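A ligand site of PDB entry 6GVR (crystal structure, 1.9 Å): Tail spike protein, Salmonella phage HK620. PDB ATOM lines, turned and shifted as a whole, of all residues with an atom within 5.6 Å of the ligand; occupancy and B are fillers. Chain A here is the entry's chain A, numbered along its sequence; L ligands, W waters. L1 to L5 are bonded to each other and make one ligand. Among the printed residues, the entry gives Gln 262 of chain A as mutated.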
ATOM      1  N   GLY A 101      36.125 -12.729  25.394  1.00  0.00           N
ATOM      2  CA  GLY A 101      35.403 -13.944  25.010  1.00  0.00           C
ATOM      3  C   GLY A 101      34.352 -13.739  23.920  1.00  0.00           C
ATOM      4  O   GLY A 101      33.837 -14.718  23.364  1.00  0.00           O
ATOM      5  N   HIS A 102      34.006 -12.477  23.612  1.00  0.00           N
ATOM      6  CA  HIS A 102      33.125 -12.137  22.545  1.00  0.00           C
ATOM      7  C   HIS A 102      33.876 -11.543  21.368  1.00  0.00           C
ATOM      8  O   HIS A 102      33.237 -10.882  20.495  1.00  0.00           O
ATOM      9  CB  HIS A 102      32.098 -11.102  23.028  1.00  0.00           C
ATOM     10  CG  HIS A 102      31.360 -11.496  24.236  1.00  0.00           C
ATOM     11  ND1 HIS A 102      30.138 -12.122  24.203  1.00  0.00           N
ATOM     12  CD2 HIS A 102      31.635 -11.302  25.544  1.00  0.00           C
ATOM     13  CE1 HIS A 102      29.698 -12.327  25.417  1.00  0.00           C
ATOM     14  NE2 HIS A 102      30.599 -11.833  26.263  1.00  0.00           N
ATOM     15  N   SER A 103      35.207 -11.726  21.325  1.00  0.00           N
ATOM     16  CA  SER A 103      36.104 -11.068  20.325  1.00  0.00           C
ATOM     17  C   SER A 103      35.873  -9.559  20.284  1.00  0.00           C
ATOM     18  O   SER A 103      35.962  -8.959  19.192  1.00  0.00           O
ATOM     19  CB  SER A 103      35.853 -11.669  18.922  1.00  0.00           C
ATOM     20  OG  SER A 103      36.138 -13.044  18.980  1.00  0.00           O
ATOM     21  N   GLN A 132      33.721  -8.143  17.254  1.00  0.00           N
ATOM     22  CA  GLN A 132      32.452  -7.510  17.635  1.00  0.00           C
ATOM     23  C   GLN A 132      32.827  -6.126  18.118  1.00  0.00           C
ATOM     24  O   GLN A 132      33.550  -5.979  19.080  1.00  0.00           O
ATOM     25  CB  GLN A 132      31.714  -8.346  18.686  1.00  0.00           C
ATOM     26  CG  GLN A 132      31.193  -9.682  18.132  1.00  0.00           C
ATOM     27  CD  GLN A 132      30.174 -10.312  19.069  1.00  0.00           C
ATOM     28  OE1 GLN A 132      29.071  -9.765  19.296  1.00  0.00           O
ATOM     29  NE2 GLN A 132      30.491 -11.515  19.587  1.00  0.00           N
ATOM     30  N   PHE A 137      28.297  -6.706  26.928  1.00  0.00           N
ATOM     31  CA  PHE A 137      28.506  -7.697  27.996  1.00  0.00           C
ATOM     32  C   PHE A 137      29.711  -7.273  28.790  1.00  0.00           C
ATOM     33  O   PHE A 137      30.613  -6.584  28.270  1.00  0.00           O
ATOM     34  CB  PHE A 137      28.689  -9.117  27.492  1.00  0.00           C
ATOM     35  CG  PHE A 137      27.518  -9.677  26.668  1.00  0.00           C
ATOM     36  CD1 PHE A 137      26.356 -10.135  27.263  1.00  0.00           C
ATOM     37  CD2 PHE A 137      27.629  -9.754  25.297  1.00  0.00           C
ATOM     38  CE1 PHE A 137      25.348 -10.697  26.466  1.00  0.00           C
ATOM     39  CE2 PHE A 137      26.652 -10.304  24.500  1.00  0.00           C
ATOM     40  CZ  PHE A 137      25.537 -10.800  25.082  1.00  0.00           C
ATOM     41  N   PRO A 142      27.758 -14.819  28.966  1.00  0.00           N
ATOM     42  CA  PRO A 142      26.591 -13.919  29.096  1.00  0.00           C
ATOM     43  C   PRO A 142      25.646 -14.189  30.266  1.00  0.00           C
ATOM     44  O   PRO A 142      25.047 -13.254  30.869  1.00  0.00           O
ATOM     45  CB  PRO A 142      25.890 -14.022  27.730  1.00  0.00           C
ATOM     46  CG  PRO A 142      26.718 -14.909  26.861  1.00  0.00           C
ATOM     47  CD  PRO A 142      27.937 -15.363  27.608  1.00  0.00           C
ATOM     48  N   LEU A 172      32.417 -15.427  13.937  1.00  0.00           N
ATOM     49  CA  LEU A 172      31.330 -14.424  14.078  1.00  0.00           C
ATOM     50  C   LEU A 172      31.891 -13.018  13.993  1.00  0.00           C
ATOM     51  O   LEU A 172      33.020 -12.729  14.439  1.00  0.00           O
ATOM     52  CB  LEU A 172      30.605 -14.577  15.386  1.00  0.00           C
ATOM     53  CG  LEU A 172      30.001 -15.940  15.628  1.00  0.00           C
ATOM     54  CD1 LEU A 172      29.641 -16.019  17.114  1.00  0.00           C
ATOM     55  CD2 LEU A 172      28.834 -16.272  14.702  1.00  0.00           C
ATOM     56  N   ASN A 174      30.263  -8.860  14.409  1.00  0.00           N
ATOM     57  CA  ASN A 174      29.141  -7.957  14.822  1.00  0.00           C
ATOM     58  C   ASN A 174      29.653  -6.498  14.809  1.00  0.00           C
ATOM     59  O   ASN A 174      30.820  -6.209  15.047  1.00  0.00           O
ATOM     60  CB  ASN A 174      28.608  -8.385  16.230  1.00  0.00           C
ATOM     61  CG  ASN A 174      27.198  -7.842  16.545  1.00  0.00           C
ATOM     62  OD1 ASN A 174      26.572  -7.127  15.726  1.00  0.00           O
ATOM     63  ND2 ASN A 174      26.657  -8.203  17.735  1.00  0.00           N
ATOM     64  N   THR A 197      28.279 -11.167  10.489  1.00  0.00           N
ATOM     65  CA  THR A 197      27.190 -12.055  10.818  1.00  0.00           C
ATOM     66  C   THR A 197      25.950 -11.151  11.118  1.00  0.00           C
ATOM     67  O   THR A 197      24.849 -11.413  10.655  1.00  0.00           O
ATOM     68  CB  THR A 197      27.504 -12.843  12.048  1.00  0.00           C
ATOM     69  OG1 THR A 197      28.750 -13.569  11.879  1.00  0.00           O
ATOM     70  CG2 THR A 197      26.400 -13.783  12.377  1.00  0.00           C
ATOM     71  N   TRP A 198      26.202 -10.132  11.876  1.00  0.00           N
ATOM     72  CA  TRP A 198      25.215  -9.083  12.232  1.00  0.00           C
ATOM     73  C   TRP A 198      25.856  -7.705  12.242  1.00  0.00           C
ATOM     74  O   TRP A 198      27.087  -7.583  12.381  1.00  0.00           O
ATOM     75  CB  TRP A 198      24.664  -9.288  13.616  1.00  0.00           C
ATOM     76  CG  TRP A 198      24.263 -10.707  14.017  1.00  0.00           C
ATOM     77  CD1 TRP A 198      23.165 -11.398  13.643  1.00  0.00           C
ATOM     78  CD2 TRP A 198      25.041 -11.598  14.842  1.00  0.00           C
ATOM     79  NE1 TRP A 198      23.160 -12.639  14.223  1.00  0.00           N
ATOM     80  CE2 TRP A 198      24.317 -12.781  14.979  1.00  0.00           C
ATOM     81  CE3 TRP A 198      26.254 -11.463  15.536  1.00  0.00           C
ATOM     82  CZ2 TRP A 198      24.778 -13.840  15.724  1.00  0.00           C
ATOM     83  CZ3 TRP A 198      26.750 -12.577  16.237  1.00  0.00           C
ATOM     84  CH2 TRP A 198      25.986 -13.713  16.359  1.00  0.00           C
ATOM     85  N   THR A 201      23.041  -6.402  17.485  1.00  0.00           N
ATOM     86  CA  THR A 201      22.194  -7.338  18.203  1.00  0.00           C
ATOM     87  C   THR A 201      21.706  -6.692  19.468  1.00  0.00           C
ATOM     88  O   THR A 201      22.468  -5.953  20.096  1.00  0.00           O
ATOM     89  CB  THR A 201      22.940  -8.601  18.594  1.00  0.00           C
ATOM     90  OG1 THR A 201      24.007  -8.320  19.501  1.00  0.00           O
ATOM     91  CG2 THR A 201      23.491  -9.294  17.380  1.00  0.00           C
ATOM     92  N   LEU A 202      20.469  -6.995  19.851  1.00  0.00           N
ATOM     93  CA  LEU A 202      19.801  -6.328  20.962  1.00  0.00           C
ATOM     94  C   LEU A 202      19.401  -7.411  21.940  1.00  0.00           C
ATOM     95  O   LEU A 202      18.847  -8.426  21.568  1.00  0.00           O
ATOM     96  CB  LEU A 202      18.572  -5.583  20.533  1.00  0.00           C
ATOM     97  CG  LEU A 202      18.664  -4.621  19.385  1.00  0.00           C
ATOM     98  CD1 LEU A 202      17.248  -4.001  19.194  1.00  0.00           C
ATOM     99  CD2 LEU A 202      19.739  -3.577  19.554  1.00  0.00           C
ATOM    100  N   GLY A 203      19.714  -7.228  23.188  1.00  0.00           N
ATOM    101  CA  GLY A 203      19.318  -8.253  24.155  1.00  0.00           C
ATOM    102  C   GLY A 203      20.193  -9.522  24.107  1.00  0.00           C
ATOM    103  O   GLY A 203      21.115  -9.667  23.220  1.00  0.00           O
ATOM    104  N   TRP A 204      19.905 -10.401  25.043  1.00  0.00           N
ATOM    105  CA  TRP A 204      20.542 -11.764  25.101  1.00  0.00           C
ATOM    106  C   TRP A 204      19.526 -12.696  25.671  1.00  0.00           C
ATOM    107  O   TRP A 204      19.154 -12.543  26.866  1.00  0.00           O
ATOM    108  CB  TRP A 204      21.842 -11.784  25.902  1.00  0.00           C
ATOM    109  CG  TRP A 204      22.362 -13.174  26.021  1.00  0.00           C
ATOM    110  CD1 TRP A 204      22.895 -13.917  25.025  1.00  0.00           C
ATOM    111  CD2 TRP A 204      22.260 -14.054  27.174  1.00  0.00           C
ATOM    112  NE1 TRP A 204      23.211 -15.202  25.480  1.00  0.00           N
ATOM    113  CE2 TRP A 204      22.796 -15.322  26.786  1.00  0.00           C
ATOM    114  CE3 TRP A 204      21.798 -13.899  28.468  1.00  0.00           C
ATOM    115  CZ2 TRP A 204      22.864 -16.393  27.639  1.00  0.00           C
ATOM    116  CZ3 TRP A 204      21.851 -14.958  29.333  1.00  0.00           C
ATOM    117  CH2 TRP A 204      22.417 -16.210  28.914  1.00  0.00           C
ATOM    118  N   ASN A 205      19.085 -13.650  24.848  1.00  0.00           N
ATOM    119  CA  ASN A 205      18.135 -14.683  25.246  1.00  0.00           C
ATOM    120  C   ASN A 205      17.007 -14.199  26.129  1.00  0.00           C
ATOM    121  O   ASN A 205      16.670 -14.759  27.176  1.00  0.00           O
ATOM    122  CB  ASN A 205      18.881 -15.850  25.845  1.00  0.00           C
ATOM    123  CG  ASN A 205      19.761 -16.569  24.841  1.00  0.00           C
ATOM    124  OD1 ASN A 205      19.887 -16.181  23.639  1.00  0.00           O
ATOM    125  ND2 ASN A 205      20.531 -17.523  25.370  1.00  0.00           N
ATOM    126  N   ASP A 229      26.266 -16.963   7.183  1.00  0.00           N
ATOM    127  CA  ASP A 229      24.896 -16.532   7.501  1.00  0.00           C
ATOM    128  C   ASP A 229      24.926 -15.100   7.962  1.00  0.00           C
ATOM    129  O   ASP A 229      25.889 -14.673   8.646  1.00  0.00           O
ATOM    130  CB  ASP A 229      24.348 -17.419   8.622  1.00  0.00           C
ATOM    131  CG  ASP A 229      22.861 -17.349   8.740  1.00  0.00           C
ATOM    132  OD1 ASP A 229      22.126 -16.588   7.967  1.00  0.00           O
ATOM    133  OD2 ASP A 229      22.458 -18.072   9.650  1.00  0.00           O
ATOM    134  N   HIS A 230      23.909 -14.340   7.621  1.00  0.00           N
ATOM    135  CA  HIS A 230      23.858 -12.965   8.032  1.00  0.00           C
ATOM    136  C   HIS A 230      22.419 -12.540   8.364  1.00  0.00           C
ATOM    137  O   HIS A 230      21.499 -12.834   7.639  1.00  0.00           O
ATOM    138  CB  HIS A 230      24.406 -12.022   6.963  1.00  0.00           C
ATOM    139  CG  HIS A 230      24.203 -10.574   7.277  1.00  0.00           C
ATOM    140  ND1 HIS A 230      25.222  -9.756   7.755  1.00  0.00           N
ATOM    141  CD2 HIS A 230      23.113  -9.786   7.125  1.00  0.00           C
ATOM    142  CE1 HIS A 230      24.721  -8.537   7.905  1.00  0.00           C
ATOM    143  NE2 HIS A 230      23.451  -8.536   7.529  1.00  0.00           N
ATOM    144  N   SER A 231      22.298 -11.848   9.494  1.00  0.00           N
ATOM    145  CA  SER A 231      21.017 -11.158   9.870  1.00  0.00           C
ATOM    146  C   SER A 231      21.423  -9.789  10.365  1.00  0.00           C
ATOM    147  O   SER A 231      22.190  -9.714  11.346  1.00  0.00           O
ATOM    148  CB  SER A 231      20.255 -11.927  10.950  1.00  0.00           C
ATOM    149  OG  SER A 231      19.745 -13.150  10.395  1.00  0.00           O
ATOM    150  N   TYR A 234      19.448  -8.350  15.062  1.00  0.00           N
ATOM    151  CA  TYR A 234      18.874  -9.494  15.781  1.00  0.00           C
ATOM    152  C   TYR A 234      18.263  -8.952  17.068  1.00  0.00           C
ATOM    153  O   TYR A 234      18.963  -8.407  17.949  1.00  0.00           O
ATOM    154  CB  TYR A 234      19.954 -10.518  16.141  1.00  0.00           C
ATOM    155  CG  TYR A 234      19.534 -11.948  16.436  1.00  0.00           C
ATOM    156  CD1 TYR A 234      18.856 -12.273  17.606  1.00  0.00           C
ATOM    157  CD2 TYR A 234      19.847 -13.008  15.569  1.00  0.00           C
ATOM    158  CE1 TYR A 234      18.501 -13.595  17.879  1.00  0.00           C
ATOM    159  CE2 TYR A 234      19.507 -14.318  15.850  1.00  0.00           C
ATOM    160  CZ  TYR A 234      18.885 -14.629  17.049  1.00  0.00           C
ATOM    161  OH  TYR A 234      18.593 -15.941  17.340  1.00  0.00           O
ATOM    162  N   ASN A 236      16.658  -9.665  20.382  1.00  0.00           N
ATOM    163  CA  ASN A 236      16.578 -10.797  21.353  1.00  0.00           C
ATOM    164  C   ASN A 236      16.243 -10.338  22.773  1.00  0.00           C
ATOM    165  O   ASN A 236      16.499 -10.997  23.796  1.00  0.00           O
ATOM    166  CB  ASN A 236      17.861 -11.593  21.319  1.00  0.00           C
ATOM    167  CG  ASN A 236      17.682 -13.059  21.692  1.00  0.00           C
ATOM    168  OD1 ASN A 236      16.574 -13.550  21.875  1.00  0.00           O
ATOM    169  ND2 ASN A 236      18.858 -13.793  21.862  1.00  0.00           N
ATOM    170  N   GLN A 262      15.819 -10.115  12.684  1.00  0.00           N
ATOM    171  CA  GLN A 262      15.327 -11.266  13.464  1.00  0.00           C
ATOM    172  C   GLN A 262      14.448 -10.709  14.595  1.00  0.00           C
ATOM    173  O   GLN A 262      15.007  -9.983  15.409  1.00  0.00           O
ATOM    174  CB  GLN A 262      16.514 -12.091  14.094  1.00  0.00           C
ATOM    175  CG  GLN A 262      17.468 -12.689  13.031  1.00  0.00           C
ATOM    176  CD  GLN A 262      16.949 -13.935  12.259  1.00  0.00           C
ATOM    177  OE1 GLN A 262      17.348 -14.133  11.077  1.00  0.00           O
ATOM    178  NE2 GLN A 262      16.144 -14.797  12.893  1.00  0.00           N
ATOM    179  N   HIS A 264      12.785 -12.033  17.852  1.00  0.00           N
ATOM    180  CA  HIS A 264      12.860 -13.297  18.573  1.00  0.00           C
ATOM    181  C   HIS A 264      12.334 -13.237  19.971  1.00  0.00           C
ATOM    182  O   HIS A 264      12.536 -14.232  20.709  1.00  0.00           O
ATOM    183  CB  HIS A 264      14.275 -13.816  18.616  1.00  0.00           C
ATOM    184  CG  HIS A 264      14.699 -14.506  17.384  1.00  0.00           C
ATOM    185  ND1 HIS A 264      15.480 -15.640  17.406  1.00  0.00           N
ATOM    186  CD2 HIS A 264      14.417 -14.277  16.083  1.00  0.00           C
ATOM    187  CE1 HIS A 264      15.695 -16.058  16.167  1.00  0.00           C
ATOM    188  NE2 HIS A 264      15.127 -15.216  15.341  1.00  0.00           N
ATOM    189  N   TYR A 283      12.784 -12.952  10.046  1.00  0.00           N
ATOM    190  CA  TYR A 283      12.322 -14.132  10.756  1.00  0.00           C
ATOM    191  C   TYR A 283      11.559 -13.670  12.012  1.00  0.00           C
ATOM    192  O   TYR A 283      12.001 -12.744  12.684  1.00  0.00           O
ATOM    193  CB  TYR A 283      13.469 -15.000  11.209  1.00  0.00           C
ATOM    194  CG  TYR A 283      14.152 -15.815  10.125  1.00  0.00           C
ATOM    195  CD1 TYR A 283      15.144 -15.241   9.324  1.00  0.00           C
ATOM    196  CD2 TYR A 283      13.847 -17.191   9.945  1.00  0.00           C
ATOM    197  CE1 TYR A 283      15.872 -16.030   8.380  1.00  0.00           C
ATOM    198  CE2 TYR A 283      14.527 -17.943   8.937  1.00  0.00           C
ATOM    199  CZ  TYR A 283      15.517 -17.349   8.164  1.00  0.00           C
ATOM    200  OH  TYR A 283      16.191 -18.115   7.215  1.00  0.00           O
ATOM    201  N   VAL A 285      10.304 -15.572  15.193  1.00  0.00           N
ATOM    202  CA  VAL A 285      10.625 -16.946  15.661  1.00  0.00           C
ATOM    203  C   VAL A 285      10.716 -16.948  17.172  1.00  0.00           C
ATOM    204  O   VAL A 285      11.409 -16.067  17.703  1.00  0.00           O
ATOM    205  CB  VAL A 285      11.997 -17.453  15.100  1.00  0.00           C
ATOM    206  CG1 VAL A 285      12.448 -18.759  15.798  1.00  0.00           C
ATOM    207  CG2 VAL A 285      11.930 -17.723  13.618  1.00  0.00           C
ATOM    208  N   HIS A 287      12.629 -19.238  19.661  1.00  0.00           N
ATOM    209  CA  HIS A 287      13.551 -20.378  19.866  1.00  0.00           C
ATOM    210  C   HIS A 287      13.472 -20.765  21.374  1.00  0.00           C
ATOM    211  O   HIS A 287      13.829 -19.978  22.237  1.00  0.00           O
ATOM    212  CB  HIS A 287      14.995 -20.012  19.566  1.00  0.00           C
ATOM    213  CG  HIS A 287      15.396 -19.957  18.115  1.00  0.00           C
ATOM    214  ND1 HIS A 287      15.101 -20.949  17.215  1.00  0.00           N
ATOM    215  CD2 HIS A 287      16.281 -19.135  17.486  1.00  0.00           C
ATOM    216  CE1 HIS A 287      15.662 -20.666  16.045  1.00  0.00           C
ATOM    217  NE2 HIS A 287      16.357 -19.549  16.171  1.00  0.00           N
ATOM    218  N   ALA A 289      15.589 -22.278  22.979  1.00  0.00           N
ATOM    219  CA  ALA A 289      16.894 -21.988  23.500  1.00  0.00           C
ATOM    220  C   ALA A 289      17.171 -20.557  23.922  1.00  0.00           C
ATOM    221  O   ALA A 289      18.164 -20.291  24.621  1.00  0.00           O
ATOM    222  CB  ALA A 289      17.966 -22.478  22.525  1.00  0.00           C
ATOM    223  N   GLU A 290      16.310 -19.614  23.563  1.00  0.00           N
ATOM    224  CA  GLU A 290      16.506 -18.242  23.857  1.00  0.00           C
ATOM    225  C   GLU A 290      15.462 -17.739  24.811  1.00  0.00           C
ATOM    226  O   GLU A 290      15.191 -16.517  24.897  1.00  0.00           O
ATOM    227  CB  GLU A 290      16.401 -17.419  22.505  1.00  0.00           C
ATOM    228  CG  GLU A 290      17.511 -17.773  21.522  1.00  0.00           C
ATOM    229  CD  GLU A 290      17.463 -16.945  20.261  1.00  0.00           C
ATOM    230  OE1 GLU A 290      16.312 -16.607  19.847  1.00  0.00           O
ATOM    231  OE2 GLU A 290      18.547 -16.711  19.698  1.00  0.00           O
ATOM    232  N   PRO A 359      11.156 -22.657  10.901  1.00  0.00           N
ATOM    233  CA  PRO A 359      12.379 -22.261  10.114  1.00  0.00           C
ATOM    234  C   PRO A 359      13.290 -23.532   9.780  1.00  0.00           C
ATOM    235  O   PRO A 359      13.505 -23.921   8.606  1.00  0.00           O
ATOM    236  CB  PRO A 359      13.100 -21.288  11.097  1.00  0.00           C
ATOM    237  CG  PRO A 359      12.625 -21.698  12.524  1.00  0.00           C
ATOM    238  CD  PRO A 359      11.494 -22.723  12.360  1.00  0.00           C
HETATM  239  C1  LIG L   1      18.767 -16.971  11.014  1.00  0.00           C
HETATM  240  C2  LIG L   1      19.715 -16.784  12.218  1.00  0.00           C
HETATM  241  C3  LIG L   1      19.732 -18.067  13.083  1.00  0.00           C
HETATM  242  C4  LIG L   1      18.289 -18.409  13.479  1.00  0.00           C
HETATM  243  C5  LIG L   1      17.394 -18.546  12.229  1.00  0.00           C
HETATM  244  C6  LIG L   1      15.936 -18.724  12.494  1.00  0.00           C
HETATM  245  C7  LIG L   1      21.696 -15.285  12.122  1.00  0.00           C
HETATM  246  C8  LIG L   1      22.968 -14.993  11.418  1.00  0.00           C
HETATM  247  O1  LIG L   1      17.461 -17.376  11.442  1.00  0.00           O
HETATM  248  O2  LIG L   1      20.509 -17.800  14.297  1.00  0.00           O
HETATM  249  O3  LIG L   1      18.162 -19.561  14.333  1.00  0.00           O
HETATM  250  O4  LIG L   1      15.551 -17.475  13.118  1.00  0.00           O
HETATM  251  O5  LIG L   1      21.308 -14.570  13.056  1.00  0.00           O
HETATM  252  N1  LIG L   1      21.023 -16.392  11.722  1.00  0.00           N
HETATM  253  O6  LIG L   1      19.234 -18.006  10.203  1.00  0.00           O
HETATM  254  C1  LG2 L   2      21.209 -18.937  14.809  1.00  0.00           C
HETATM  255  C2  LG2 L   2      21.443 -18.646  16.273  1.00  0.00           C
HETATM  256  C3  LG2 L   2      22.382 -17.438  16.500  1.00  0.00           C
HETATM  257  C4  LG2 L   2      23.638 -17.561  15.633  1.00  0.00           C
HETATM  258  C5  LG2 L   2      23.246 -17.838  14.170  1.00  0.00           C
HETATM  259  C6  LG2 L   2      24.396 -18.057  13.202  1.00  0.00           C
HETATM  260  O1  LG2 L   2      20.174 -18.394  16.920  1.00  0.00           O
HETATM  261  O2  LG2 L   2      22.685 -17.419  17.904  1.00  0.00           O
HETATM  262  O3  LG2 L   2      24.435 -18.679  16.110  1.00  0.00           O
HETATM  263  O4  LG2 L   2      22.388 -18.996  14.111  1.00  0.00           O
HETATM  264  O5  LG2 L   2      25.262 -16.939  13.303  1.00  0.00           O
HETATM  265  C1  LG3 L   3      25.835 -18.304  16.260  1.00  0.00           C
HETATM  266  C2  LG3 L   3      26.685 -19.576  16.510  1.00  0.00           C
HETATM  267  C3  LG3 L   3      26.314 -20.296  17.808  1.00  0.00           C
HETATM  268  C4  LG3 L   3      26.500 -19.292  18.882  1.00  0.00           C
HETATM  269  C5  LG3 L   3      25.631 -18.061  18.624  1.00  0.00           C
HETATM  270  C6  LG3 L   3      25.758 -16.991  19.719  1.00  0.00           C
HETATM  271  O1  LG3 L   3      26.532 -20.440  15.460  1.00  0.00           O
HETATM  272  O2  LG3 L   3      27.261 -21.326  18.015  1.00  0.00           O
HETATM  273  O3  LG3 L   3      26.245 -19.908  20.115  1.00  0.00           O
HETATM  274  O4  LG3 L   3      26.022 -17.446  17.359  1.00  0.00           O
HETATM  275  O5  LG3 L   3      27.124 -16.485  19.853  1.00  0.00           O
HETATM  276  C1  LG4 L   4      22.105 -16.295  18.568  1.00  0.00           C
HETATM  277  C2  LG4 L   4      22.057 -16.602  20.057  1.00  0.00           C
HETATM  278  C3  LG4 L   4      21.569 -15.416  20.874  1.00  0.00           C
HETATM  279  C4  LG4 L   4      22.211 -14.126  20.472  1.00  0.00           C
HETATM  280  C5  LG4 L   4      22.075 -14.010  18.992  1.00  0.00           C
HETATM  281  C6  LG4 L   4      22.569 -12.685  18.514  1.00  0.00           C
HETATM  282  C7  LG4 L   4      21.610 -18.885  20.750  1.00  0.00           C
HETATM  283  C8  LG4 L   4      20.630 -20.037  20.848  1.00  0.00           C
HETATM  284  N1  LG4 L   4      21.185 -17.729  20.222  1.00  0.00           N
HETATM  285  O1  LG4 L   4      21.918 -15.709  22.190  1.00  0.00           O
HETATM  286  O2  LG4 L   4      21.456 -13.072  21.081  1.00  0.00           O
HETATM  287  O3  LG4 L   4      22.809 -15.073  18.332  1.00  0.00           O
HETATM  288  O4  LG4 L   4      23.945 -12.665  18.727  1.00  0.00           O
HETATM  289  O5  LG4 L   4      22.731 -18.996  21.215  1.00  0.00           O
HETATM  290  C1  LG5 L   5      27.639 -16.773  21.177  1.00  0.00           C
HETATM  291  C2  LG5 L   5      29.148 -16.515  21.148  1.00  0.00           C
HETATM  292  C3  LG5 L   5      29.484 -15.035  21.002  1.00  0.00           C
HETATM  293  C4  LG5 L   5      28.664 -14.231  22.029  1.00  0.00           C
HETATM  294  C5  LG5 L   5      27.175 -14.637  22.021  1.00  0.00           C
HETATM  295  C6  LG5 L   5      26.323 -13.961  23.114  1.00  0.00           C
HETATM  296  O1  LG5 L   5      29.597 -17.051  22.379  1.00  0.00           O
HETATM  297  O2  LG5 L   5      30.921 -14.833  21.121  1.00  0.00           O
HETATM  298  O3  LG5 L   5      28.906 -12.829  21.812  1.00  0.00           O
HETATM  299  O4  LG5 L   5      27.001 -16.045  22.219  1.00  0.00           O
HETATM  300  O   HOH W   1      26.861 -23.206  19.982  1.00  0.00           O
HETATM  301  O   HOH W   2      23.135 -11.514  22.553  1.00  0.00           O
HETATM  302  O   HOH W   3      19.425 -21.004  17.469  1.00  0.00           O
HETATM  303  O   HOH W   4      32.756 -14.062  18.926  1.00  0.00           O
HETATM  304  O   HOH W   5      23.817 -21.489  15.184  1.00  0.00           O
HETATM  305  O   HOH W   6      27.539 -10.670  21.026  1.00  0.00           O
HETATM  306  O   HOH W   7      19.050 -18.057   7.587  1.00  0.00           O
HETATM  307  O   HOH W   8      24.839 -10.735  20.613  1.00  0.00           O
HETATM  308  O   HOH W   9      22.654 -18.908  23.979  1.00  0.00           O
HETATM  309  O   HOH W  10      30.960 -15.573  24.847  1.00  0.00           O
HETATM  310  O   HOH W  11      28.841 -20.378  14.246  1.00  0.00           O
HETATM  311  O   HOH W  12      29.049 -19.677  22.198  1.00  0.00           O
HETATM  312  O   HOH W  13      27.128 -17.516  11.398  1.00  0.00           O
HETATM  313  O   HOH W  14      18.689 -21.946  13.568  1.00  0.00           O
HETATM  314  O   HOH W  15      24.362 -16.845  23.278  1.00  0.00           O
HETATM  315  O   HOH W  16      32.792 -16.755  21.295  1.00  0.00           O
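A ring nitrogen (NE2) of His 264 is in hydrogen-bond range of an oxygen (O4) of LIG L1 (3.2 Å). OE2 of Glu 290 lies within hydrogen-bond range of N1 of LG4 L4. A nitrogen (N1) of LIG L1 sits at hydrogen-bond distance from the side-chain carboxylate (OD2) of Asp 229, 3.0 Å away. OH of Tyr 234 is in hydrogen-bond range of O1 of LG2 L2, 2.9 Å away. A ring nitrogen (ND1) of His 102 lies within hydrogen-bond range of an oxygen (O3) of LG5 L5 (2.8 Å). An oxygen (O1) of LG4 L4 sits at hydrogen-bond distance from the side-chain amide oxygen (OD1) of Asn 205. NE2 of Gln 262 is in hydrogen-bond range of O4 of LIG L1 (2.8 Å). O3 of LG5 L5 is in hydrogen-bond range of NE2 of Gln 132 (3.0 Å). An oxygen (O5) of LIG L1 is in hydrogen-bond range of the indole nitrogen of Trp 198, at 2.9 Å. An oxygen (O3) of LIG L1 is in hydrogen-bond range of a ring nitrogen (NE2) of His 287 (2.6 Å). The side-chain amide nitrogen (ND2) of Asn 236 sits at hydrogen-bond distance from an oxygen (O2) of LG4 L4. O5 of LIG L1 lies close to OG of Ser 231 (3.4 Å).
The backbone carbonyl oxygen (O) of Tyr 234 is in hydrogen-bond range of the backbone NH (N) of Leu 202 (2.8 Å). NE2 of Gln 262 lies within hydrogen-bond range of NE2 of His 264, at 2.7 Å. The side-chain carboxylate (OE2) of Glu 290 is in hydrogen-bond range of the side-chain hydroxyl (OH) of Tyr 234 (2.5 Å). The backbone NH of Gln 132 is in hydrogen-bond range of the backbone carbonyl oxygen of Ser 103 (3.1 Å). OG of Ser 231 lies within hydrogen-bond range of OE1 of Gln 262 (2.7 Å). OG1 of Thr 201 sits at hydrogen-bond distance from ND2 of Asn 174 (3.2 Å). The side-chain hydroxyl of Tyr 234 lies within hydrogen-bond range of a ring nitrogen (ND1) of His 264, at 3.1 Å. O of Trp 198 sits close to OD1 of Asn 174, at 3.4 Å.
O of Gly 101 touches O2 of LG5 L5, 3.7 Å away. CZ of Phe 137 touches C6 of LG5 L5, at 3.8 Å. CG of Pro 142 touches C6 of LG5 L5, 3.9 Å away. CD1 of Leu 172 touches O5 of LG3 L3, 3.7 Å away. CG2 of Thr 197 touches O5 of LG2 L2, at 3.5 Å. CG2 of Thr 201 touches O4 of LG4 L4 (3.7 Å). CD1 of Trp 204 touches O1 of LG4 L4 (3.5 Å). His 230 touches the ligand. CD2 of Tyr 283 touches O4 of LIG L1, 3.6 Å away. Val 285 touches the ligand. CB of Ala 289 touches C8 of LG4 L4 (3.98 Å). Hydrophobic or aromatic side chains that line the ligand: His 102, Phe 137, Pro 142, Leu 172, Trp 198, Trp 204, Tyr 234, His 264, Tyr 283, Val 285, His 287 and Ala 289. Of the 28 residues printed, 23 come within 4 Å of the ligand.
Water W7 lies within hydrogen-bond range of an oxygen (O6) of LIG L1 (2.6 Å), the side-chain hydroxyl of Tyr 283 (2.9 Å) and the side-chain carboxylate of Asp 229 (3.4 Å). Water W6 lies within hydrogen-bond range of the side-chain amide oxygen of Gln 132 and an oxygen (O3) of LG5 L5. Water W2 lies within hydrogen-bond range of O2 of LG4 L4 and O of Gly 203. Water W9 bridges an oxygen (O5) of LG4 L4 (2.8 Å) and the side-chain amide nitrogen of Asn 205 (2.9 Å). Water W15 lies within hydrogen-bond range of an oxygen (O1) of LG4 L4 and the indole nitrogen (NE1) of Trp 204. Water W10 lies within hydrogen-bond range of an oxygen (O1) of LG5 L5 (3.2 Å) and the backbone carbonyl oxygen of Gly 101 (3.3 Å).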
